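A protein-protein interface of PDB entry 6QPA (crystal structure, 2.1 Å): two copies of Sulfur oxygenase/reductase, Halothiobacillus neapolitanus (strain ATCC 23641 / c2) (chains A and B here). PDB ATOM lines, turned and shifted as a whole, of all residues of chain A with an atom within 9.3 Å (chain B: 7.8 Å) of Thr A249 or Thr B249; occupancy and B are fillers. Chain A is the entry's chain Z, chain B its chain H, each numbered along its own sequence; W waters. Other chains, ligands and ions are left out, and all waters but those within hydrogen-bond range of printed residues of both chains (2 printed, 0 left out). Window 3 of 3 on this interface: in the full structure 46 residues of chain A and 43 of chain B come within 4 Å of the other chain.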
ATOM      1  N   TRP A 115     -13.490 -10.897 -20.711  1.00  0.00           N
ATOM      2  CA  TRP A 115     -13.746  -9.733 -19.883  1.00  0.00           C
ATOM      3  C   TRP A 115     -13.251 -10.100 -18.496  1.00  0.00           C
ATOM      4  O   TRP A 115     -13.595 -11.173 -17.990  1.00  0.00           O
ATOM      5  CB  TRP A 115     -15.238  -9.406 -19.895  1.00  0.00           C
ATOM      6  CG  TRP A 115     -15.625  -8.159 -19.199  1.00  0.00           C
ATOM      7  CD1 TRP A 115     -16.404  -8.064 -18.082  1.00  0.00           C
ATOM      8  CD2 TRP A 115     -15.293  -6.811 -19.578  1.00  0.00           C
ATOM      9  NE1 TRP A 115     -16.576  -6.740 -17.736  1.00  0.00           N
ATOM     10  CE2 TRP A 115     -15.910  -5.949 -18.638  1.00  0.00           C
ATOM     11  CE3 TRP A 115     -14.551  -6.246 -20.623  1.00  0.00           C
ATOM     12  CZ2 TRP A 115     -15.782  -4.551 -18.691  1.00  0.00           C
ATOM     13  CZ3 TRP A 115     -14.422  -4.832 -20.676  1.00  0.00           C
ATOM     14  CH2 TRP A 115     -15.045  -4.017 -19.718  1.00  0.00           C
ATOM     15  N   HIS A 165     -25.511 -11.555  -9.162  1.00  0.00           N
ATOM     16  CA  HIS A 165     -26.438 -10.617  -8.535  1.00  0.00           C
ATOM     17  C   HIS A 165     -26.062  -9.187  -8.906  1.00  0.00           C
ATOM     18  O   HIS A 165     -24.891  -8.806  -8.796  1.00  0.00           O
ATOM     19  CB  HIS A 165     -26.439 -10.759  -7.002  1.00  0.00           C
ATOM     20  CG  HIS A 165     -26.794 -12.126  -6.503  1.00  0.00           C
ATOM     21  ND1 HIS A 165     -25.961 -13.217  -6.640  1.00  0.00           N
ATOM     22  CD2 HIS A 165     -27.886 -12.570  -5.835  1.00  0.00           C
ATOM     23  CE1 HIS A 165     -26.535 -14.276  -6.096  1.00  0.00           C
ATOM     24  NE2 HIS A 165     -27.699 -13.909  -5.593  1.00  0.00           N
ATOM     25  N   TRP A 166     -27.047  -8.397  -9.340  1.00  0.00           N
ATOM     26  CA  TRP A 166     -26.898  -6.945  -9.436  1.00  0.00           C
ATOM     27  C   TRP A 166     -27.699  -6.302  -8.312  1.00  0.00           C
ATOM     28  O   TRP A 166     -28.927  -6.461  -8.245  1.00  0.00           O
ATOM     29  CB  TRP A 166     -27.366  -6.403 -10.784  1.00  0.00           C
ATOM     30  CG  TRP A 166     -26.594  -6.892 -11.979  1.00  0.00           C
ATOM     31  CD1 TRP A 166     -25.695  -7.919 -12.023  1.00  0.00           C
ATOM     32  CD2 TRP A 166     -26.660  -6.356 -13.312  1.00  0.00           C
ATOM     33  NE1 TRP A 166     -25.210  -8.062 -13.304  1.00  0.00           N
ATOM     34  CE2 TRP A 166     -25.785  -7.113 -14.111  1.00  0.00           C
ATOM     35  CE3 TRP A 166     -27.372  -5.296 -13.900  1.00  0.00           C
ATOM     36  CZ2 TRP A 166     -25.598  -6.848 -15.476  1.00  0.00           C
ATOM     37  CZ3 TRP A 166     -27.191  -5.036 -15.258  1.00  0.00           C
ATOM     38  CH2 TRP A 166     -26.312  -5.809 -16.025  1.00  0.00           C
ATOM     39  N   VAL A 167     -27.018  -5.528  -7.473  1.00  0.00           N
ATOM     40  CA  VAL A 167     -27.597  -5.002  -6.247  1.00  0.00           C
ATOM     41  C   VAL A 167     -27.995  -3.541  -6.461  1.00  0.00           C
ATOM     42  O   VAL A 167     -27.261  -2.763  -7.085  1.00  0.00           O
ATOM     43  CB  VAL A 167     -26.601  -5.190  -5.083  1.00  0.00           C
ATOM     44  CG1 VAL A 167     -27.056  -4.476  -3.802  1.00  0.00           C
ATOM     45  CG2 VAL A 167     -26.407  -6.692  -4.828  1.00  0.00           C
ATOM     46  N   MET A 168     -29.181  -3.183  -5.974  1.00  0.00           N
ATOM     47  CA  MET A 168     -29.695  -1.830  -6.091  1.00  0.00           C
ATOM     48  C   MET A 168     -28.763  -0.822  -5.434  1.00  0.00           C
ATOM     49  O   MET A 168     -28.274  -1.028  -4.318  1.00  0.00           O
ATOM     50  CB  MET A 168     -31.068  -1.738  -5.429  1.00  0.00           C
ATOM     51  CG  MET A 168     -32.119  -2.662  -6.052  1.00  0.00           C
ATOM     52  SD  MET A 168     -33.522  -2.888  -4.940  1.00  0.00           S
ATOM     53  CE  MET A 168     -34.252  -1.230  -4.886  1.00  0.00           C
ATOM     54  N   ASP A 169     -28.585   0.301  -6.113  1.00  0.00           N
ATOM     55  CA  ASP A 169     -27.799   1.415  -5.592  1.00  0.00           C
ATOM     56  C   ASP A 169     -28.194   1.726  -4.158  1.00  0.00           C
ATOM     57  O   ASP A 169     -29.366   1.968  -3.864  1.00  0.00           O
ATOM     58  CB  ASP A 169     -28.040   2.623  -6.492  1.00  0.00           C
ATOM     59  CG  ASP A 169     -27.168   3.829  -6.114  1.00  0.00           C
ATOM     60  OD1 ASP A 169     -26.184   3.677  -5.376  1.00  0.00           O
ATOM     61  OD2 ASP A 169     -27.475   4.932  -6.568  1.00  0.00           O
ATOM     62  N   GLY A 170     -27.208   1.686  -3.263  1.00  0.00           N
ATOM     63  CA  GLY A 170     -27.416   1.943  -1.854  1.00  0.00           C
ATOM     64  C   GLY A 170     -27.775   0.738  -1.014  1.00  0.00           C
ATOM     65  O   GLY A 170     -27.869   0.859   0.214  1.00  0.00           O
ATOM     66  N   GLU A 172     -25.952  -2.120  -1.003  1.00  0.00           N
ATOM     67  CA  GLU A 172     -24.808  -3.029  -1.020  1.00  0.00           C
ATOM     68  C   GLU A 172     -24.595  -3.691   0.337  1.00  0.00           C
ATOM     69  O   GLU A 172     -24.437  -4.912   0.429  1.00  0.00           O
ATOM     70  CB  GLU A 172     -23.545  -2.278  -1.456  1.00  0.00           C
ATOM     71  CG  GLU A 172     -23.390  -2.086  -2.961  1.00  0.00           C
ATOM     72  CD  GLU A 172     -24.097  -0.838  -3.498  1.00  0.00           C
ATOM     73  OE1 GLU A 172     -24.840  -0.182  -2.738  1.00  0.00           O
ATOM     74  OE2 GLU A 172     -23.879  -0.497  -4.685  1.00  0.00           O
ATOM     75  N   LYS A 200     -17.251  -9.049  -4.734  1.00  0.00           N
ATOM     76  CA  LYS A 200     -17.813  -7.778  -5.160  1.00  0.00           C
ATOM     77  C   LYS A 200     -16.947  -7.210  -6.272  1.00  0.00           C
ATOM     78  O   LYS A 200     -15.745  -7.010  -6.081  1.00  0.00           O
ATOM     79  CB  LYS A 200     -17.894  -6.793  -3.991  1.00  0.00           C
ATOM     80  CG  LYS A 200     -18.539  -5.477  -4.356  1.00  0.00           C
ATOM     81  CD  LYS A 200     -18.350  -4.478  -3.189  1.00  0.00           C
ATOM     82  CE  LYS A 200     -19.032  -3.140  -3.427  1.00  0.00           C
ATOM     83  NZ  LYS A 200     -18.655  -2.203  -2.333  1.00  0.00           N
ATOM     84  N   GLN A 201     -17.546  -6.949  -7.428  1.00  0.00           N
ATOM     85  CA  GLN A 201     -16.779  -6.351  -8.513  1.00  0.00           C
ATOM     86  C   GLN A 201     -16.498  -4.881  -8.208  1.00  0.00           C
ATOM     87  O   GLN A 201     -17.422  -4.118  -7.933  1.00  0.00           O
ATOM     88  CB  GLN A 201     -17.535  -6.477  -9.835  1.00  0.00           C
ATOM     89  CG  GLN A 201     -16.785  -5.764 -10.951  1.00  0.00           C
ATOM     90  CD  GLN A 201     -17.561  -5.645 -12.247  1.00  0.00           C
ATOM     91  OE1 GLN A 201     -17.438  -4.646 -12.940  1.00  0.00           O
ATOM     92  NE2 GLN A 201     -18.353  -6.669 -12.586  1.00  0.00           N
ATOM     93  N   PHE A 202     -15.226  -4.474  -8.280  1.00  0.00           N
ATOM     94  CA  PHE A 202     -14.870  -3.077  -8.053  1.00  0.00           C
ATOM     95  C   PHE A 202     -14.071  -2.456  -9.194  1.00  0.00           C
ATOM     96  O   PHE A 202     -13.661  -1.304  -9.066  1.00  0.00           O
ATOM     97  CB  PHE A 202     -14.092  -2.916  -6.729  1.00  0.00           C
ATOM     98  CG  PHE A 202     -12.706  -3.569  -6.713  1.00  0.00           C
ATOM     99  CD1 PHE A 202     -12.552  -4.907  -6.378  1.00  0.00           C
ATOM    100  CD2 PHE A 202     -11.557  -2.809  -6.973  1.00  0.00           C
ATOM    101  CE1 PHE A 202     -11.259  -5.505  -6.356  1.00  0.00           C
ATOM    102  CE2 PHE A 202     -10.284  -3.378  -6.943  1.00  0.00           C
ATOM    103  CZ  PHE A 202     -10.130  -4.731  -6.632  1.00  0.00           C
ATOM    104  N   GLY A 203     -13.849  -3.169 -10.294  1.00  0.00           N
ATOM    105  CA  GLY A 203     -13.111  -2.635 -11.426  1.00  0.00           C
ATOM    106  C   GLY A 203     -12.844  -3.736 -12.435  1.00  0.00           C
ATOM    107  O   GLY A 203     -13.192  -4.900 -12.229  1.00  0.00           O
ATOM    108  N   VAL A 204     -12.226  -3.344 -13.548  1.00  0.00           N
ATOM    109  CA  VAL A 204     -11.924  -4.273 -14.632  1.00  0.00           C
ATOM    110  C   VAL A 204     -10.517  -3.989 -15.154  1.00  0.00           C
ATOM    111  O   VAL A 204     -10.078  -2.832 -15.203  1.00  0.00           O
ATOM    112  CB  VAL A 204     -12.966  -4.178 -15.769  1.00  0.00           C
ATOM    113  CG1 VAL A 204     -12.676  -5.217 -16.873  1.00  0.00           C
ATOM    114  CG2 VAL A 204     -14.418  -4.359 -15.222  1.00  0.00           C
ATOM    115  N   ILE A 245     -10.423   0.402 -15.573  1.00  0.00           N
ATOM    116  CA  ILE A 245     -11.828   0.459 -15.954  1.00  0.00           C
ATOM    117  C   ILE A 245     -12.662   0.385 -14.685  1.00  0.00           C
ATOM    118  O   ILE A 245     -12.477  -0.528 -13.872  1.00  0.00           O
ATOM    119  CB  ILE A 245     -12.181  -0.675 -16.926  1.00  0.00           C
ATOM    120  CG1 ILE A 245     -11.384  -0.517 -18.224  1.00  0.00           C
ATOM    121  CG2 ILE A 245     -13.700  -0.721 -17.179  1.00  0.00           C
ATOM    122  CD1 ILE A 245     -11.479  -1.740 -19.125  1.00  0.00           C
ATOM    123  N   PRO A 246     -13.579   1.319 -14.479  1.00  0.00           N
ATOM    124  CA  PRO A 246     -14.411   1.298 -13.270  1.00  0.00           C
ATOM    125  C   PRO A 246     -15.295   0.059 -13.194  1.00  0.00           C
ATOM    126  O   PRO A 246     -15.657  -0.547 -14.211  1.00  0.00           O
ATOM    127  CB  PRO A 246     -15.260   2.573 -13.401  1.00  0.00           C
ATOM    128  CG  PRO A 246     -14.527   3.421 -14.395  1.00  0.00           C
ATOM    129  CD  PRO A 246     -13.833   2.493 -15.326  1.00  0.00           C
ATOM    130  N   GLY A 247     -15.629  -0.325 -11.964  1.00  0.00           N
ATOM    131  CA  GLY A 247     -16.639  -1.348 -11.774  1.00  0.00           C
ATOM    132  C   GLY A 247     -17.982  -0.920 -12.335  1.00  0.00           C
ATOM    133  O   GLY A 247     -18.330   0.266 -12.359  1.00  0.00           O
ATOM    134  N   GLN A 248     -18.746  -1.904 -12.800  1.00  0.00           N
ATOM    135  CA  GLN A 248     -20.053  -1.601 -13.354  1.00  0.00           C
ATOM    136  C   GLN A 248     -21.024  -1.183 -12.253  1.00  0.00           C
ATOM    137  O   GLN A 248     -20.879  -1.550 -11.083  1.00  0.00           O
ATOM    138  CB  GLN A 248     -20.612  -2.813 -14.093  1.00  0.00           C
ATOM    139  CG  GLN A 248     -21.059  -3.908 -13.138  1.00  0.00           C
ATOM    140  CD  GLN A 248     -21.963  -4.900 -13.806  1.00  0.00           C
ATOM    141  OE1 GLN A 248     -21.508  -5.736 -14.586  1.00  0.00           O
ATOM    142  NE2 GLN A 248     -23.271  -4.806 -13.516  1.00  0.00           N
ATOM    143  N   THR A 249     -22.011  -0.389 -12.632  1.00  0.00           N
ATOM    144  CA  THR A 249     -23.162  -0.196 -11.768  1.00  0.00           C
ATOM    145  C   THR A 249     -24.401  -0.581 -12.557  1.00  0.00           C
ATOM    146  O   THR A 249     -24.424  -0.406 -13.779  1.00  0.00           O
ATOM    147  CB  THR A 249     -23.319   1.244 -11.256  1.00  0.00           C
ATOM    148  OG1 THR A 249     -23.762   2.098 -12.319  1.00  0.00           O
ATOM    149  CG2 THR A 249     -21.959   1.769 -10.702  1.00  0.00           C
ATOM    150  N   PRO A 250     -25.433  -1.147 -11.909  1.00  0.00           N
ATOM    151  CA  PRO A 250     -25.517  -1.527 -10.491  1.00  0.00           C
ATOM    152  C   PRO A 250     -24.391  -2.503 -10.054  1.00  0.00           C
ATOM    153  O   PRO A 250     -23.943  -3.318 -10.854  1.00  0.00           O
ATOM    154  CB  PRO A 250     -26.885  -2.219 -10.399  1.00  0.00           C
ATOM    155  CG  PRO A 250     -27.678  -1.686 -11.570  1.00  0.00           C
ATOM    156  CD  PRO A 250     -26.679  -1.462 -12.650  1.00  0.00           C
ATOM    157  N   THR A 251     -23.965  -2.417  -8.799  1.00  0.00           N
ATOM    158  CA  THR A 251     -22.860  -3.235  -8.320  1.00  0.00           C
ATOM    159  C   THR A 251     -23.124  -4.721  -8.559  1.00  0.00           C
ATOM    160  O   THR A 251     -24.173  -5.251  -8.184  1.00  0.00           O
ATOM    161  CB  THR A 251     -22.636  -2.976  -6.831  1.00  0.00           C
ATOM    162  OG1 THR A 251     -22.483  -1.566  -6.608  1.00  0.00           O
ATOM    163  CG2 THR A 251     -21.359  -3.698  -6.348  1.00  0.00           C
ATOM    164  N   GLN A 252     -22.165  -5.399  -9.181  1.00  0.00           N
ATOM    165  CA  GLN A 252     -22.268  -6.844  -9.366  1.00  0.00           C
ATOM    166  C   GLN A 252     -21.628  -7.570  -8.189  1.00  0.00           C
ATOM    167  O   GLN A 252     -20.501  -7.247  -7.791  1.00  0.00           O
ATOM    168  CB  GLN A 252     -21.604  -7.306 -10.664  1.00  0.00           C
ATOM    169  CG  GLN A 252     -21.574  -8.858 -10.790  1.00  0.00           C
ATOM    170  CD  GLN A 252     -20.857  -9.337 -12.040  1.00  0.00           C
ATOM    171  OE1 GLN A 252     -19.674  -9.016 -12.260  1.00  0.00           O
ATOM    172  NE2 GLN A 252     -21.570 -10.105 -12.875  1.00  0.00           N
ATOM    173  N   ASP A 291     -31.432  -5.568  -8.355  1.00  0.00           N
ATOM    174  CA  ASP A 291     -31.908  -5.142  -9.663  1.00  0.00           C
ATOM    175  C   ASP A 291     -31.957  -6.294 -10.659  1.00  0.00           C
ATOM    176  O   ASP A 291     -32.792  -6.288 -11.563  1.00  0.00           O
ATOM    177  CB  ASP A 291     -30.999  -4.053 -10.237  1.00  0.00           C
ATOM    178  CG  ASP A 291     -31.289  -2.686  -9.664  1.00  0.00           C
ATOM    179  OD1 ASP A 291     -32.466  -2.423  -9.330  1.00  0.00           O
ATOM    180  OD2 ASP A 291     -30.328  -1.885  -9.559  1.00  0.00           O
ATOM    181  N   TRP B 166     -19.602  -0.456 -24.679  1.00  0.00           N
ATOM    182  CA  TRP B 166     -19.618   0.227 -23.392  1.00  0.00           C
ATOM    183  C   TRP B 166     -18.674   1.419 -23.486  1.00  0.00           C
ATOM    184  O   TRP B 166     -17.487   1.243 -23.764  1.00  0.00           O
ATOM    185  CB  TRP B 166     -19.173  -0.686 -22.251  1.00  0.00           C
ATOM    186  CG  TRP B 166     -20.058  -1.828 -21.985  1.00  0.00           C
ATOM    187  CD1 TRP B 166     -21.080  -2.279 -22.766  1.00  0.00           C
ATOM    188  CD2 TRP B 166     -19.997  -2.697 -20.854  1.00  0.00           C
ATOM    189  NE1 TRP B 166     -21.670  -3.376 -22.185  1.00  0.00           N
ATOM    190  CE2 TRP B 166     -21.024  -3.656 -21.011  1.00  0.00           C
ATOM    191  CE3 TRP B 166     -19.171  -2.758 -19.719  1.00  0.00           C
ATOM    192  CZ2 TRP B 166     -21.253  -4.671 -20.076  1.00  0.00           C
ATOM    193  CZ3 TRP B 166     -19.394  -3.759 -18.796  1.00  0.00           C
ATOM    194  CH2 TRP B 166     -20.429  -4.707 -18.979  1.00  0.00           C
ATOM    195  N   VAL B 167     -19.192   2.619 -23.221  1.00  0.00           N
ATOM    196  CA  VAL B 167     -18.462   3.855 -23.470  1.00  0.00           C
ATOM    197  C   VAL B 167     -17.872   4.379 -22.168  1.00  0.00           C
ATOM    198  O   VAL B 167     -18.525   4.347 -21.118  1.00  0.00           O
ATOM    199  CB  VAL B 167     -19.379   4.888 -24.145  1.00  0.00           C
ATOM    200  CG1 VAL B 167     -18.704   6.287 -24.266  1.00  0.00           C
ATOM    201  CG2 VAL B 167     -19.794   4.368 -25.512  1.00  0.00           C
ATOM    202  N   ASP B 169     -16.691   6.644 -19.187  1.00  0.00           N
ATOM    203  CA  ASP B 169     -17.306   7.766 -18.500  1.00  0.00           C
ATOM    204  C   ASP B 169     -16.780   9.085 -19.060  1.00  0.00           C
ATOM    205  O   ASP B 169     -15.566   9.294 -19.159  1.00  0.00           O
ATOM    206  CB  ASP B 169     -17.005   7.661 -17.003  1.00  0.00           C
ATOM    207  CG  ASP B 169     -17.770   8.679 -16.187  1.00  0.00           C
ATOM    208  OD1 ASP B 169     -18.747   9.241 -16.720  1.00  0.00           O
ATOM    209  OD2 ASP B 169     -17.415   8.910 -15.016  1.00  0.00           O
ATOM    210  N   GLU B 172     -19.316   9.984 -23.789  1.00  0.00           N
ATOM    211  CA  GLU B 172     -20.566   9.647 -24.469  1.00  0.00           C
ATOM    212  C   GLU B 172     -20.770  10.489 -25.724  1.00  0.00           C
ATOM    213  O   GLU B 172     -21.083   9.961 -26.796  1.00  0.00           O
ATOM    214  CB  GLU B 172     -21.753   9.813 -23.517  1.00  0.00           C
ATOM    215  CG  GLU B 172     -21.989   8.654 -22.538  1.00  0.00           C
ATOM    216  CD  GLU B 172     -21.135   8.761 -21.283  1.00  0.00           C
ATOM    217  OE1 GLU B 172     -20.239   9.634 -21.229  1.00  0.00           O
ATOM    218  OE2 GLU B 172     -21.380   7.992 -20.334  1.00  0.00           O
ATOM    219  N   GLN B 201     -28.671   3.084 -23.875  1.00  0.00           N
ATOM    220  CA  GLN B 201     -29.424   2.564 -22.731  1.00  0.00           C
ATOM    221  C   GLN B 201     -29.511   3.604 -21.616  1.00  0.00           C
ATOM    222  O   GLN B 201     -28.487   4.117 -21.171  1.00  0.00           O
ATOM    223  CB  GLN B 201     -28.778   1.296 -22.166  1.00  0.00           C
ATOM    224  CG  GLN B 201     -29.492   0.820 -20.903  1.00  0.00           C
ATOM    225  CD  GLN B 201     -28.785  -0.309 -20.169  1.00  0.00           C
ATOM    226  OE1 GLN B 201     -28.838  -0.385 -18.945  1.00  0.00           O
ATOM    227  NE2 GLN B 201     -28.142  -1.195 -20.911  1.00  0.00           N
ATOM    228  N   PRO B 246     -31.999   1.941 -12.900  1.00  0.00           N
ATOM    229  CA  PRO B 246     -31.119   2.876 -13.629  1.00  0.00           C
ATOM    230  C   PRO B 246     -30.411   2.204 -14.796  1.00  0.00           C
ATOM    231  O   PRO B 246     -30.204   0.989 -14.813  1.00  0.00           O
ATOM    232  CB  PRO B 246     -30.116   3.341 -12.560  1.00  0.00           C
ATOM    233  CG  PRO B 246     -30.775   3.033 -11.245  1.00  0.00           C
ATOM    234  CD  PRO B 246     -31.645   1.817 -11.477  1.00  0.00           C
ATOM    235  N   GLY B 247     -30.070   3.001 -15.802  1.00  0.00           N
ATOM    236  CA  GLY B 247     -29.202   2.499 -16.852  1.00  0.00           C
ATOM    237  C   GLY B 247     -27.853   2.090 -16.292  1.00  0.00           C
ATOM    238  O   GLY B 247     -27.355   2.671 -15.327  1.00  0.00           O
ATOM    239  N   GLN B 248     -27.252   1.076 -16.910  1.00  0.00           N
ATOM    240  CA  GLN B 248     -25.964   0.608 -16.431  1.00  0.00           C
ATOM    241  C   GLN B 248     -24.875   1.635 -16.712  1.00  0.00           C
ATOM    242  O   GLN B 248     -24.983   2.450 -17.631  1.00  0.00           O
ATOM    243  CB  GLN B 248     -25.587  -0.709 -17.104  1.00  0.00           C
ATOM    244  CG  GLN B 248     -25.178  -0.538 -18.538  1.00  0.00           C
ATOM    245  CD  GLN B 248     -24.447  -1.759 -19.057  1.00  0.00           C
ATOM    246  OE1 GLN B 248     -23.203  -1.787 -19.102  1.00  0.00           O
ATOM    247  NE2 GLN B 248     -25.206  -2.776 -19.446  1.00  0.00           N
ATOM    248  N   THR B 249     -23.817   1.592 -15.899  1.00  0.00           N
ATOM    249  CA  THR B 249     -22.561   2.251 -16.215  1.00  0.00           C
ATOM    250  C   THR B 249     -21.448   1.205 -16.237  1.00  0.00           C
ATOM    251  O   THR B 249     -21.502   0.235 -15.475  1.00  0.00           O
ATOM    252  CB  THR B 249     -22.199   3.364 -15.209  1.00  0.00           C
ATOM    253  OG1 THR B 249     -21.832   2.788 -13.948  1.00  0.00           O
ATOM    254  CG2 THR B 249     -23.383   4.328 -15.016  1.00  0.00           C
ATOM    255  N   PRO B 250     -20.440   1.345 -17.126  1.00  0.00           N
ATOM    256  CA  PRO B 250     -20.295   2.364 -18.181  1.00  0.00           C
ATOM    257  C   PRO B 250     -21.483   2.347 -19.157  1.00  0.00           C
ATOM    258  O   PRO B 250     -22.105   1.299 -19.353  1.00  0.00           O
ATOM    259  CB  PRO B 250     -19.006   1.955 -18.898  1.00  0.00           C
ATOM    260  CG  PRO B 250     -18.265   1.128 -17.921  1.00  0.00           C
ATOM    261  CD  PRO B 250     -19.299   0.402 -17.118  1.00  0.00           C
ATOM    262  N   THR B 251     -21.818   3.493 -19.730  1.00  0.00           N
ATOM    263  CA  THR B 251     -22.987   3.580 -20.605  1.00  0.00           C
ATOM    264  C   THR B 251     -22.919   2.579 -21.755  1.00  0.00           C
ATOM    265  O   THR B 251     -21.897   2.469 -22.440  1.00  0.00           O
ATOM    266  CB  THR B 251     -23.101   4.989 -21.162  1.00  0.00           C
ATOM    267  OG1 THR B 251     -23.101   5.898 -20.066  1.00  0.00           O
ATOM    268  CG2 THR B 251     -24.398   5.126 -21.958  1.00  0.00           C
ATOM    269  N   GLN B 252     -24.008   1.837 -21.959  1.00  0.00           N
ATOM    270  CA  GLN B 252     -24.110   0.934 -23.096  1.00  0.00           C
ATOM    271  C   GLN B 252     -24.780   1.632 -24.271  1.00  0.00           C
ATOM    272  O   GLN B 252     -25.858   2.220 -24.123  1.00  0.00           O
ATOM    273  CB  GLN B 252     -24.912  -0.324 -22.759  1.00  0.00           C
ATOM    274  CG  GLN B 252     -25.120  -1.230 -23.985  1.00  0.00           C
ATOM    275  CD  GLN B 252     -26.012  -2.424 -23.670  1.00  0.00           C
ATOM    276  OE1 GLN B 252     -27.146  -2.249 -23.214  1.00  0.00           O
ATOM    277  NE2 GLN B 252     -25.514  -3.636 -23.916  1.00  0.00           N
ATOM    278  N   ASP B 291     -14.816   1.339 -23.121  1.00  0.00           N
ATOM    279  CA  ASP B 291     -14.374   0.407 -22.092  1.00  0.00           C
ATOM    280  C   ASP B 291     -14.516  -1.040 -22.547  1.00  0.00           C
ATOM    281  O   ASP B 291     -13.710  -1.880 -22.141  1.00  0.00           O
ATOM    282  CB  ASP B 291     -15.181   0.581 -20.810  1.00  0.00           C
ATOM    283  CG  ASP B 291     -14.693   1.729 -19.959  1.00  0.00           C
ATOM    284  OD1 ASP B 291     -13.482   2.008 -19.959  1.00  0.00           O
ATOM    285  OD2 ASP B 291     -15.540   2.346 -19.282  1.00  0.00           O
HETATM  286  O   HOH W   1     -26.397   2.234 -12.677  1.00  0.00           O
HETATM  287  O   HOH W   2     -19.250   2.427 -13.985  1.00  0.00           O
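Of the printed residues of chain B, Thr A249 touches Gln B248 (3.2 Å) and Thr B249 (2.6 Å). Thr B249 touches two residues of chain A. No residue of chain B comes within 4 Å of Pro A250. No residue of chain A comes within 4 Å of Pro B250. Printed residues of chain A within 4 Å of Gln B248: Thr A249. Of the printed residues of chain A, Trp B166 touches Trp A115. Of the printed residues of chain B, Gln A248 touches Thr B249 (3.2 Å). Of the printed residues of chain B, Ile A245 touches Asp B291. Of the printed residues of chain A, Asp B291 touches Trp A115 and Ile A245. Thr A251 touches none of the printed residues of chain B. The nearest residue of chain A that does not touch Thr B249 is Gly A247 (4.4 Å).
Water W2 lies within hydrogen-bond range of OG1 of Thr B249 (2.6 Å) and O of Gly A247 (2.9 Å). Water W1 bridges the side-chain hydroxyl (OG1) of Thr A249 and the backbone carbonyl oxygen (O) of Gly B247.
OG1 of Thr A249 lies within hydrogen-bond range of OG1 of Thr B249, 2.6 Å away.
Gln A248 touches Thr B249, and with the chains exchanged Thr A249 touches Gln B248. Thr B249 touches its own counterpart, Thr A249. Of the 6 pairs that touch across the chains among the printed residues, 3 have their exchanged pair printed and touching as well.
Among the printed residues, pairs that only touch across the chains: Gln A248 with Thr B249, Thr A249 with Gln B248, Trp A115 with Asp B291, Trp A115 with Trp B166 and Ile A245 with Asp B291.
N of Asp B291 lies within hydrogen-bond range of O of Trp B166. The side-chain amide oxygen (OE1) of Gln B201 sits at hydrogen-bond distance from the backbone NH (N) of Gln B248, at 3.0 Å. The side-chain amide oxygen of Gln B248 sits close to the backbone carbonyl oxygen of Pro B250, 3.3 Å away. OE1 of Gln A201 is in hydrogen-bond range of N of Gln A248, 3.0 Å away. The backbone NH of Val A204 is in hydrogen-bond range of the backbone carbonyl oxygen of Ile A245, at 2.8 Å. The backbone carbonyl oxygen (O) of Pro A250 is in hydrogen-bond range of the side-chain amide nitrogen (NE2) of Gln A248 (3.1 Å).
Printed residues of chain B that touch a printed residue of chain A: Trp B166, Gln B248, Thr B249 and Asp B291. Hydrophobic or aromatic side chains of chain B that line the printed part of chain A: Trp B166. Along chain B the printed residues that touch a printed residue of chain A span positions 166 to 291. Of the 22 printed residues of chain A, 4 touch a printed residue of chain B. Hydrophobic or aromatic side chains of chain A that line the printed part of chain B: Trp A115 and Ile A245. Among the printed residues, no Asp or Glu carboxylate lies within 4 Å of a Lys or Arg side-chain nitrogen of the other chain.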
